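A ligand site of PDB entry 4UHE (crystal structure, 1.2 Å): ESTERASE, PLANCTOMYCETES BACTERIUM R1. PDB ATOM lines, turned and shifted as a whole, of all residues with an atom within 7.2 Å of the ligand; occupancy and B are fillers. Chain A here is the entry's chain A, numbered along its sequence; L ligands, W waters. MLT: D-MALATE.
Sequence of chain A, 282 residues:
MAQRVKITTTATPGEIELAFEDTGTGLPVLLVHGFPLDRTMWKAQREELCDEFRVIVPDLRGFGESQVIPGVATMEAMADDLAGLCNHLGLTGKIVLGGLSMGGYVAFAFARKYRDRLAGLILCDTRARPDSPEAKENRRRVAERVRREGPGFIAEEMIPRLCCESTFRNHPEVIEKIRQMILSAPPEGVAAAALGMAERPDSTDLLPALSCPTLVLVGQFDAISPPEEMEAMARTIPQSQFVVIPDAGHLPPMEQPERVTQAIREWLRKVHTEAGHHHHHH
NE2 of His 250 sits at hydrogen-bond distance from O1 of the ligand (2.8 Å).
O1 of the ligand lies close to OG of Ser 101 (2.9 Å).
An oxygen (O5) of the ligand is in hydrogen-bond range of the side-chain hydroxyl of Tyr 105.
O4 of the ligand is in salt-bridge range of NH1 of Arg 139, at 2.8 Å.
O2 of the ligand sits at hydrogen-bond distance from N of Phe 35, at 2.8 Å.
An oxygen (O2) of the ligand lies within hydrogen-bond range of the backbone NH (N) of Met 102, at 2.9 Å.
The backbone NH (N) of His 250 lies within hydrogen-bond range of the backbone carbonyl oxygen (O) of Leu 162 (3.0 Å).
OG of Ser 101 lies within hydrogen-bond range of NE2 of His 250 (2.9 Å).
The side-chain hydroxyl (OG) of Ser 225 sits at hydrogen-bond distance from a ring nitrogen (ND1) of His 250 (3.2 Å).
The backbone NH (N) of Ser 101 lies close to the backbone carbonyl oxygen (O) of Asp 125.
The guanidinium group (NE) of Arg 139 is in salt-bridge range of the side-chain carboxylate (OD2) of Asp 131, at 2.8 Å.
The backbone carbonyl oxygen of Met 197 lies within hydrogen-bond range of the guanidinium group of Arg 200, 2.9 Å away.
The side-chain hydroxyl (OG1) of Thr 126 sits at hydrogen-bond distance from the backbone carbonyl oxygen (O) of Ser 101, at 2.8 Å.
Residues that only touch the ligand: Gly 34 (3.8 Å), Met 158 (3.7 Å), Met 197 (3.9 Å) and Ile 224 (3.8 Å).
Within 4 Å of the ligand: Gly 34, Phe 35, Ser 101, Met 102, Tyr 105, Arg 139, Met 158, Met 197, Ile 224 and His 250.
Water W1 bridges an oxygen (O3) of the ligand (2.8 Å) and the guanidinium group (NH2) of Arg 161 (3.0 Å).
Water W4 bridges O1 of the ligand (2.8 Å) and O of Phe 35 (3.0 Å).
Water W3 lies within hydrogen-bond range of O5 of the ligand and OH of Tyr 105.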
ATOM      1  N   HIS A  33     -15.590  -4.544  -4.607  1.00  0.00           N
ATOM      2  CA  HIS A  33     -15.172  -3.313  -5.238  1.00  0.00           C
ATOM      3  C   HIS A  33     -15.613  -3.188  -6.687  1.00  0.00           C
ATOM      4  O   HIS A  33     -15.997  -4.133  -7.346  1.00  0.00           O
ATOM      5  CB  HIS A  33     -13.645  -3.168  -5.138  1.00  0.00           C
ATOM      6  CG  HIS A  33     -12.849  -4.203  -5.892  1.00  0.00           C
ATOM      7  ND1 HIS A  33     -12.604  -4.127  -7.244  1.00  0.00           N
ATOM      8  CD2 HIS A  33     -12.203  -5.326  -5.479  1.00  0.00           C
ATOM      9  CE1 HIS A  33     -11.885  -5.171  -7.602  1.00  0.00           C
ATOM     10  NE2 HIS A  33     -11.650  -5.931  -6.553  1.00  0.00           N
ATOM     11  N   GLY A  34     -15.464  -1.958  -7.210  1.00  0.00           N
ATOM     12  CA  GLY A  34     -15.723  -1.613  -8.598  1.00  0.00           C
ATOM     13  C   GLY A  34     -14.564  -1.830  -9.532  1.00  0.00           C
ATOM     14  O   GLY A  34     -13.451  -2.182  -9.138  1.00  0.00           O
ATOM     15  N   PHE A  35     -14.823  -1.529 -10.797  1.00  0.00           N
ATOM     16  CA  PHE A  35     -13.825  -1.627 -11.845  1.00  0.00           C
ATOM     17  C   PHE A  35     -13.153  -0.265 -12.079  1.00  0.00           C
ATOM     18  O   PHE A  35     -13.868   0.744 -12.164  1.00  0.00           O
ATOM     19  CB  PHE A  35     -14.492  -2.025 -13.163  1.00  0.00           C
ATOM     20  CG  PHE A  35     -13.608  -2.007 -14.382  1.00  0.00           C
ATOM     21  CD1 PHE A  35     -12.925  -3.137 -14.765  1.00  0.00           C
ATOM     22  CD2 PHE A  35     -13.560  -0.894 -15.177  1.00  0.00           C
ATOM     23  CE1 PHE A  35     -12.165  -3.166 -15.910  1.00  0.00           C
ATOM     24  CE2 PHE A  35     -12.768  -0.878 -16.339  1.00  0.00           C
ATOM     25  CZ  PHE A  35     -12.117  -2.035 -16.706  1.00  0.00           C
ATOM     26  N   PRO A  36     -11.849  -0.205 -12.301  1.00  0.00           N
ATOM     27  CA  PRO A  36     -10.806  -1.234 -12.127  1.00  0.00           C
ATOM     28  C   PRO A  36     -10.054  -0.925 -10.815  1.00  0.00           C
ATOM     29  O   PRO A  36      -8.929  -0.446 -10.830  1.00  0.00           O
ATOM     30  CB  PRO A  36      -9.921  -1.002 -13.342  1.00  0.00           C
ATOM     31  CG  PRO A  36      -9.942   0.486 -13.562  1.00  0.00           C
ATOM     32  CD  PRO A  36     -11.259   0.987 -12.931  1.00  0.00           C
ATOM     33  N   LEU A  37     -10.749  -1.130  -9.698  1.00  0.00           N
ATOM     34  CA  LEU A  37     -10.253  -0.727  -8.394  1.00  0.00           C
ATOM     35  C   LEU A  37      -9.768  -1.944  -7.618  1.00  0.00           C
ATOM     36  O   LEU A  37      -9.316  -2.914  -8.229  1.00  0.00           O
ATOM     37  CB  LEU A  37     -11.296   0.119  -7.655  1.00  0.00           C
ATOM     38  CG  LEU A  37     -11.879   1.298  -8.424  1.00  0.00           C
ATOM     39  CD1 LEU A  37     -12.854   2.081  -7.522  1.00  0.00           C
ATOM     40  CD2 LEU A  37     -10.822   2.199  -8.995  1.00  0.00           C
ATOM     41  N   LEU A 100     -20.267  -2.501  -5.515  1.00  0.00           N
ATOM     42  CA  LEU A 100     -20.319  -1.216  -6.172  1.00  0.00           C
ATOM     43  C   LEU A 100     -20.013  -1.397  -7.660  1.00  0.00           C
ATOM     44  O   LEU A 100     -18.968  -1.937  -8.004  1.00  0.00           O
ATOM     45  CB  LEU A 100     -19.375  -0.218  -5.517  1.00  0.00           C
ATOM     46  CG  LEU A 100     -19.462   1.190  -6.161  1.00  0.00           C
ATOM     47  CD1 LEU A 100     -19.410   2.296  -5.136  1.00  0.00           C
ATOM     48  CD2 LEU A 100     -18.426   1.402  -7.238  1.00  0.00           C
ATOM     49  N   SER A 101     -20.943  -0.948  -8.513  1.00  0.00           N
ATOM     50  CA  SER A 101     -20.789  -0.894  -9.965  1.00  0.00           C
ATOM     51  C   SER A 101     -20.504  -2.251 -10.559  1.00  0.00           C
ATOM     52  O   SER A 101     -21.380  -3.108 -10.511  1.00  0.00           O
ATOM     53  CB  SER A 101     -19.893   0.257 -10.345  1.00  0.00           C
ATOM     54  OG  SER A 101     -20.089   0.601 -11.730  1.00  0.00           O
ATOM     55  N   MET A 102     -19.280  -2.528 -11.094  1.00  0.00           N
ATOM     56  CA  MET A 102     -18.989  -3.906 -11.471  1.00  0.00           C
ATOM     57  C   MET A 102     -19.236  -4.904 -10.352  1.00  0.00           C
ATOM     58  O   MET A 102     -19.668  -6.033 -10.585  1.00  0.00           O
ATOM     59  CB  MET A 102     -17.554  -4.028 -12.004  1.00  0.00           C
ATOM     60  CG  MET A 102     -17.213  -5.420 -12.487  1.00  0.00           C
ATOM     61  SD  MET A 102     -15.519  -5.677 -13.005  1.00  0.00           S
ATOM     62  CE  MET A 102     -14.727  -5.748 -11.472  1.00  0.00           C
ATOM     63  N   GLY A 103     -18.905  -4.492  -9.125  1.00  0.00           N
ATOM     64  CA  GLY A 103     -19.171  -5.351  -8.012  1.00  0.00           C
ATOM     65  C   GLY A 103     -20.663  -5.661  -7.844  1.00  0.00           C
ATOM     66  O   GLY A 103     -21.028  -6.716  -7.309  1.00  0.00           O
ATOM     67  N   GLY A 104     -21.533  -4.698  -8.233  1.00  0.00           N
ATOM     68  CA  GLY A 104     -22.960  -4.973  -8.335  1.00  0.00           C
ATOM     69  C   GLY A 104     -23.318  -5.995  -9.397  1.00  0.00           C
ATOM     70  O   GLY A 104     -24.152  -6.861  -9.177  1.00  0.00           O
ATOM     71  N   TYR A 105     -22.617  -5.941 -10.525  1.00  0.00           N
ATOM     72  CA  TYR A 105     -22.822  -6.984 -11.540  1.00  0.00           C
ATOM     73  C   TYR A 105     -22.456  -8.368 -11.002  1.00  0.00           C
ATOM     74  O   TYR A 105     -23.143  -9.362 -11.279  1.00  0.00           O
ATOM     75  CB  TYR A 105     -21.981  -6.745 -12.813  1.00  0.00           C
ATOM     76  CG  TYR A 105     -22.056  -5.372 -13.461  1.00  0.00           C
ATOM     77  CD1 TYR A 105     -23.117  -4.505 -13.270  1.00  0.00           C
ATOM     78  CD2 TYR A 105     -21.043  -4.970 -14.259  1.00  0.00           C
ATOM     79  CE1 TYR A 105     -23.132  -3.219 -13.849  1.00  0.00           C
ATOM     80  CE2 TYR A 105     -21.017  -3.721 -14.867  1.00  0.00           C
ATOM     81  CZ  TYR A 105     -22.049  -2.836 -14.621  1.00  0.00           C
ATOM     82  OH  TYR A 105     -22.033  -1.556 -15.138  1.00  0.00           O
ATOM     83  N   ASP A 125     -24.468   2.063  -6.827  1.00  0.00           N
ATOM     84  CA  ASP A 125     -23.912   2.692  -8.032  1.00  0.00           C
ATOM     85  C   ASP A 125     -23.694   1.675  -9.151  1.00  0.00           C
ATOM     86  O   ASP A 125     -22.581   1.460  -9.627  1.00  0.00           O
ATOM     87  CB  ASP A 125     -22.615   3.449  -7.681  1.00  0.00           C
ATOM     88  CG  ASP A 125     -22.825   4.396  -6.551  1.00  0.00           C
ATOM     89  OD1 ASP A 125     -22.712   4.046  -5.387  1.00  0.00           O
ATOM     90  OD2 ASP A 125     -23.233   5.618  -6.806  1.00  0.00           O
ATOM     91  N   THR A 126     -24.815   1.028  -9.548  1.00  0.00           N
ATOM     92  CA  THR A 126     -24.755  -0.086 -10.476  1.00  0.00           C
ATOM     93  C   THR A 126     -26.041  -0.139 -11.306  1.00  0.00           C
ATOM     94  O   THR A 126     -26.914   0.727 -11.155  1.00  0.00           O
ATOM     95  CB  THR A 126     -24.486  -1.399  -9.683  1.00  0.00           C
ATOM     96  OG1 THR A 126     -24.137  -2.458 -10.595  1.00  0.00           O
ATOM     97  CG2 THR A 126     -25.669  -1.790  -8.856  1.00  0.00           C
ATOM     98  N   ARG A 127     -26.125  -1.143 -12.166  1.00  0.00           N
ATOM     99  CA  ARG A 127     -27.262  -1.340 -13.026  1.00  0.00           C
ATOM    100  C   ARG A 127     -27.417  -2.808 -13.351  1.00  0.00           C
ATOM    101  O   ARG A 127     -26.424  -3.561 -13.355  1.00  0.00           O
ATOM    102  CB  ARG A 127     -27.247  -0.528 -14.279  1.00  0.00           C
ATOM    103  CG  ARG A 127     -26.187  -0.823 -15.262  1.00  0.00           C
ATOM    104  CD  ARG A 127     -25.961   0.451 -16.104  1.00  0.00           C
ATOM    105  NE  ARG A 127     -27.055   0.748 -17.038  1.00  0.00           N
ATOM    106  CZ  ARG A 127     -27.177   0.283 -18.288  1.00  0.00           C
ATOM    107  NH1 ARG A 127     -26.261  -0.568 -18.804  1.00  0.00           N
ATOM    108  NH2 ARG A 127     -28.250   0.634 -19.033  1.00  0.00           N
ATOM    109  N   ASP A 131     -24.533  -4.614 -21.196  1.00  0.00           N
ATOM    110  CA  ASP A 131     -23.973  -3.622 -22.107  1.00  0.00           C
ATOM    111  C   ASP A 131     -24.789  -3.570 -23.400  1.00  0.00           C
ATOM    112  O   ASP A 131     -25.183  -4.617 -23.937  1.00  0.00           O
ATOM    113  CB  ASP A 131     -22.552  -4.007 -22.494  1.00  0.00           C
ATOM    114  CG  ASP A 131     -21.495  -3.672 -21.478  1.00  0.00           C
ATOM    115  OD1 ASP A 131     -21.793  -2.983 -20.458  1.00  0.00           O
ATOM    116  OD2 ASP A 131     -20.338  -4.052 -21.743  1.00  0.00           O
ATOM    117  N   ARG A 139     -15.660  -2.200 -24.608  1.00  0.00           N
ATOM    118  CA  ARG A 139     -14.918  -3.099 -23.726  1.00  0.00           C
ATOM    119  C   ARG A 139     -13.792  -3.791 -24.419  1.00  0.00           C
ATOM    120  O   ARG A 139     -12.697  -3.950 -23.874  1.00  0.00           O
ATOM    121  CB  ARG A 139     -15.785  -4.219 -23.113  1.00  0.00           C
ATOM    122  CG  ARG A 139     -17.034  -3.882 -22.446  1.00  0.00           C
ATOM    123  CD  ARG A 139     -16.813  -3.004 -21.275  1.00  0.00           C
ATOM    124  NE  ARG A 139     -18.113  -2.866 -20.505  1.00  0.00           N
ATOM    125  CZ  ARG A 139     -18.284  -2.128 -19.416  1.00  0.00           C
ATOM    126  NH1 ARG A 139     -17.235  -1.534 -18.865  1.00  0.00           N
ATOM    127  NH2 ARG A 139     -19.485  -1.956 -18.889  1.00  0.00           N
ATOM    128  N   MET A 158     -11.751   7.922 -16.859  1.00  0.00           N
ATOM    129  CA  MET A 158     -12.736   7.587 -15.814  1.00  0.00           C
ATOM    130  C   MET A 158     -12.711   8.562 -14.669  1.00  0.00           C
ATOM    131  O   MET A 158     -13.777   8.811 -14.094  1.00  0.00           O
ATOM    132  CB  MET A 158     -12.482   6.183 -15.251  1.00  0.00           C
ATOM    133  CG  MET A 158     -12.863   4.985 -16.177  1.00  0.00           C
ATOM    134  SD  MET A 158     -12.880   3.387 -15.353  1.00  0.00           S
ATOM    135  CE  MET A 158     -14.362   3.459 -14.361  1.00  0.00           C
ATOM    136  N   ARG A 161     -15.366  11.166 -14.396  1.00  0.00           N
ATOM    137  CA  ARG A 161     -16.706  10.579 -14.321  1.00  0.00           C
ATOM    138  C   ARG A 161     -16.950   9.844 -13.020  1.00  0.00           C
ATOM    139  O   ARG A 161     -18.109   9.485 -12.748  1.00  0.00           O
ATOM    140  CB  ARG A 161     -16.915   9.597 -15.510  1.00  0.00           C
ATOM    141  CG  ARG A 161     -16.569  10.208 -16.849  1.00  0.00           C
ATOM    142  CD  ARG A 161     -17.006   9.326 -18.012  1.00  0.00           C
ATOM    143  NE  ARG A 161     -16.267   8.061 -17.997  1.00  0.00           N
ATOM    144  CZ  ARG A 161     -16.778   6.851 -17.733  1.00  0.00           C
ATOM    145  NH1 ARG A 161     -18.040   6.656 -17.509  1.00  0.00           N
ATOM    146  NH2 ARG A 161     -16.021   5.805 -17.690  1.00  0.00           N
ATOM    147  N   LEU A 162     -15.911   9.604 -12.218  1.00  0.00           N
ATOM    148  CA  LEU A 162     -16.048   8.806 -11.028  1.00  0.00           C
ATOM    149  C   LEU A 162     -16.474   9.565  -9.793  1.00  0.00           C
ATOM    150  O   LEU A 162     -17.062   8.961  -8.895  1.00  0.00           O
ATOM    151  CB  LEU A 162     -14.733   8.053 -10.744  1.00  0.00           C
ATOM    152  CG  LEU A 162     -14.487   6.803 -11.568  1.00  0.00           C
ATOM    153  CD1 LEU A 162     -13.046   6.316 -11.376  1.00  0.00           C
ATOM    154  CD2 LEU A 162     -15.451   5.712 -11.171  1.00  0.00           C
ATOM    155  N   MET A 197     -17.386  -8.063 -18.437  1.00  0.00           N
ATOM    156  CA  MET A 197     -18.507  -7.167 -18.385  1.00  0.00           C
ATOM    157  C   MET A 197     -19.290  -7.162 -19.685  1.00  0.00           C
ATOM    158  O   MET A 197     -20.505  -7.107 -19.682  1.00  0.00           O
ATOM    159  CB  MET A 197     -18.079  -5.764 -17.971  1.00  0.00           C
ATOM    160  CG  MET A 197     -17.694  -5.627 -16.515  1.00  0.00           C
ATOM    161  SD  MET A 197     -17.418  -3.963 -15.930  1.00  0.00           S
ATOM    162  CE  MET A 197     -15.779  -3.671 -16.604  1.00  0.00           C
ATOM    163  N   ARG A 200     -21.765 -10.126 -19.839  1.00  0.00           N
ATOM    164  CA  ARG A 200     -22.674 -10.388 -18.741  1.00  0.00           C
ATOM    165  C   ARG A 200     -24.104 -10.375 -19.236  1.00  0.00           C
ATOM    166  O   ARG A 200     -24.480  -9.632 -20.157  1.00  0.00           O
ATOM    167  CB  ARG A 200     -22.491  -9.395 -17.599  1.00  0.00           C
ATOM    168  CG  ARG A 200     -23.124  -8.050 -17.799  1.00  0.00           C
ATOM    169  CD  ARG A 200     -22.771  -7.085 -16.687  1.00  0.00           C
ATOM    170  NE  ARG A 200     -23.422  -5.802 -16.810  1.00  0.00           N
ATOM    171  CZ  ARG A 200     -23.055  -4.832 -17.630  1.00  0.00           C
ATOM    172  NH1 ARG A 200     -21.987  -4.934 -18.395  1.00  0.00           N
ATOM    173  NH2 ARG A 200     -23.779  -3.707 -17.690  1.00  0.00           N
ATOM    174  N   ILE A 224     -22.137   7.894 -13.831  1.00  0.00           N
ATOM    175  CA  ILE A 224     -21.983   6.608 -14.519  1.00  0.00           C
ATOM    176  C   ILE A 224     -23.223   5.748 -14.371  1.00  0.00           C
ATOM    177  O   ILE A 224     -23.668   5.123 -15.340  1.00  0.00           O
ATOM    178  CB  ILE A 224     -20.709   5.884 -14.005  1.00  0.00           C
ATOM    179  CG1 ILE A 224     -19.481   6.689 -14.397  1.00  0.00           C
ATOM    180  CG2 ILE A 224     -20.669   4.448 -14.479  1.00  0.00           C
ATOM    181  CD1 ILE A 224     -18.189   6.144 -13.834  1.00  0.00           C
ATOM    182  N   SER A 225     -23.798   5.725 -13.174  1.00  0.00           N
ATOM    183  CA  SER A 225     -25.075   5.047 -12.865  1.00  0.00           C
ATOM    184  C   SER A 225     -25.951   6.078 -12.203  1.00  0.00           C
ATOM    185  O   SER A 225     -25.949   6.165 -10.972  1.00  0.00           O
ATOM    186  CB  SER A 225     -24.842   3.805 -11.993  1.00  0.00           C
ATOM    187  OG  SER A 225     -24.006   4.079 -10.918  1.00  0.00           O
ATOM    188  N   HIS A 250     -19.934   8.608  -8.311  1.00  0.00           N
ATOM    189  CA  HIS A 250     -20.009   7.169  -8.488  1.00  0.00           C
ATOM    190  C   HIS A 250     -19.359   6.362  -7.400  1.00  0.00           C
ATOM    191  O   HIS A 250     -19.632   5.159  -7.306  1.00  0.00           O
ATOM    192  CB  HIS A 250     -19.421   6.813  -9.855  1.00  0.00           C
ATOM    193  CG  HIS A 250     -19.642   5.392 -10.278  1.00  0.00           C
ATOM    194  ND1 HIS A 250     -20.902   4.867 -10.535  1.00  0.00           N
ATOM    195  CD2 HIS A 250     -18.767   4.419 -10.612  1.00  0.00           C
ATOM    196  CE1 HIS A 250     -20.787   3.632 -10.950  1.00  0.00           C
ATOM    197  NE2 HIS A 250     -19.506   3.355 -11.039  1.00  0.00           N
ATOM    198  N   LEU A 251     -18.533   7.008  -6.564  1.00  0.00           N
ATOM    199  CA  LEU A 251     -17.819   6.308  -5.497  1.00  0.00           C
ATOM    200  C   LEU A 251     -18.175   6.820  -4.096  1.00  0.00           C
ATOM    201  O   LEU A 251     -17.280   7.162  -3.328  1.00  0.00           O
ATOM    202  CB  LEU A 251     -16.307   6.316  -5.741  1.00  0.00           C
ATOM    203  CG  LEU A 251     -15.855   5.659  -7.037  1.00  0.00           C
ATOM    204  CD1 LEU A 251     -14.353   5.887  -7.230  1.00  0.00           C
ATOM    205  CD2 LEU A 251     -16.200   4.206  -7.129  1.00  0.00           C
HETATM  206  C1  MLT L   1     -17.406   0.543 -12.372  1.00  0.00           C
HETATM  207  O1  MLT L   1     -17.360   1.649 -11.720  1.00  0.00           O
HETATM  208  O2  MLT L   1     -17.259  -0.615 -11.874  1.00  0.00           O
HETATM  209  C2  MLT L   1     -17.568   0.642 -13.861  1.00  0.00           C
HETATM  210  O3  MLT L   1     -17.798   2.018 -14.219  1.00  0.00           O
HETATM  211  C3  MLT L   1     -18.674  -0.268 -14.394  1.00  0.00           C
HETATM  212  C4  MLT L   1     -18.771  -0.322 -15.877  1.00  0.00           C
HETATM  213  O4  MLT L   1     -17.772  -0.028 -16.581  1.00  0.00           O
HETATM  214  O5  MLT L   1     -19.858  -0.706 -16.388  1.00  0.00           O
HETATM  215  O   HOH W   1     -17.603   3.485 -16.552  1.00  0.00           O
HETATM  216  O   HOH W   2     -18.673   1.800 -18.647  1.00  0.00           O
HETATM  217  O   HOH W   3     -21.817   1.309 -16.994  1.00  0.00           O
HETATM  218  O   HOH W   4     -15.380   1.767  -9.792  1.00  0.00           O
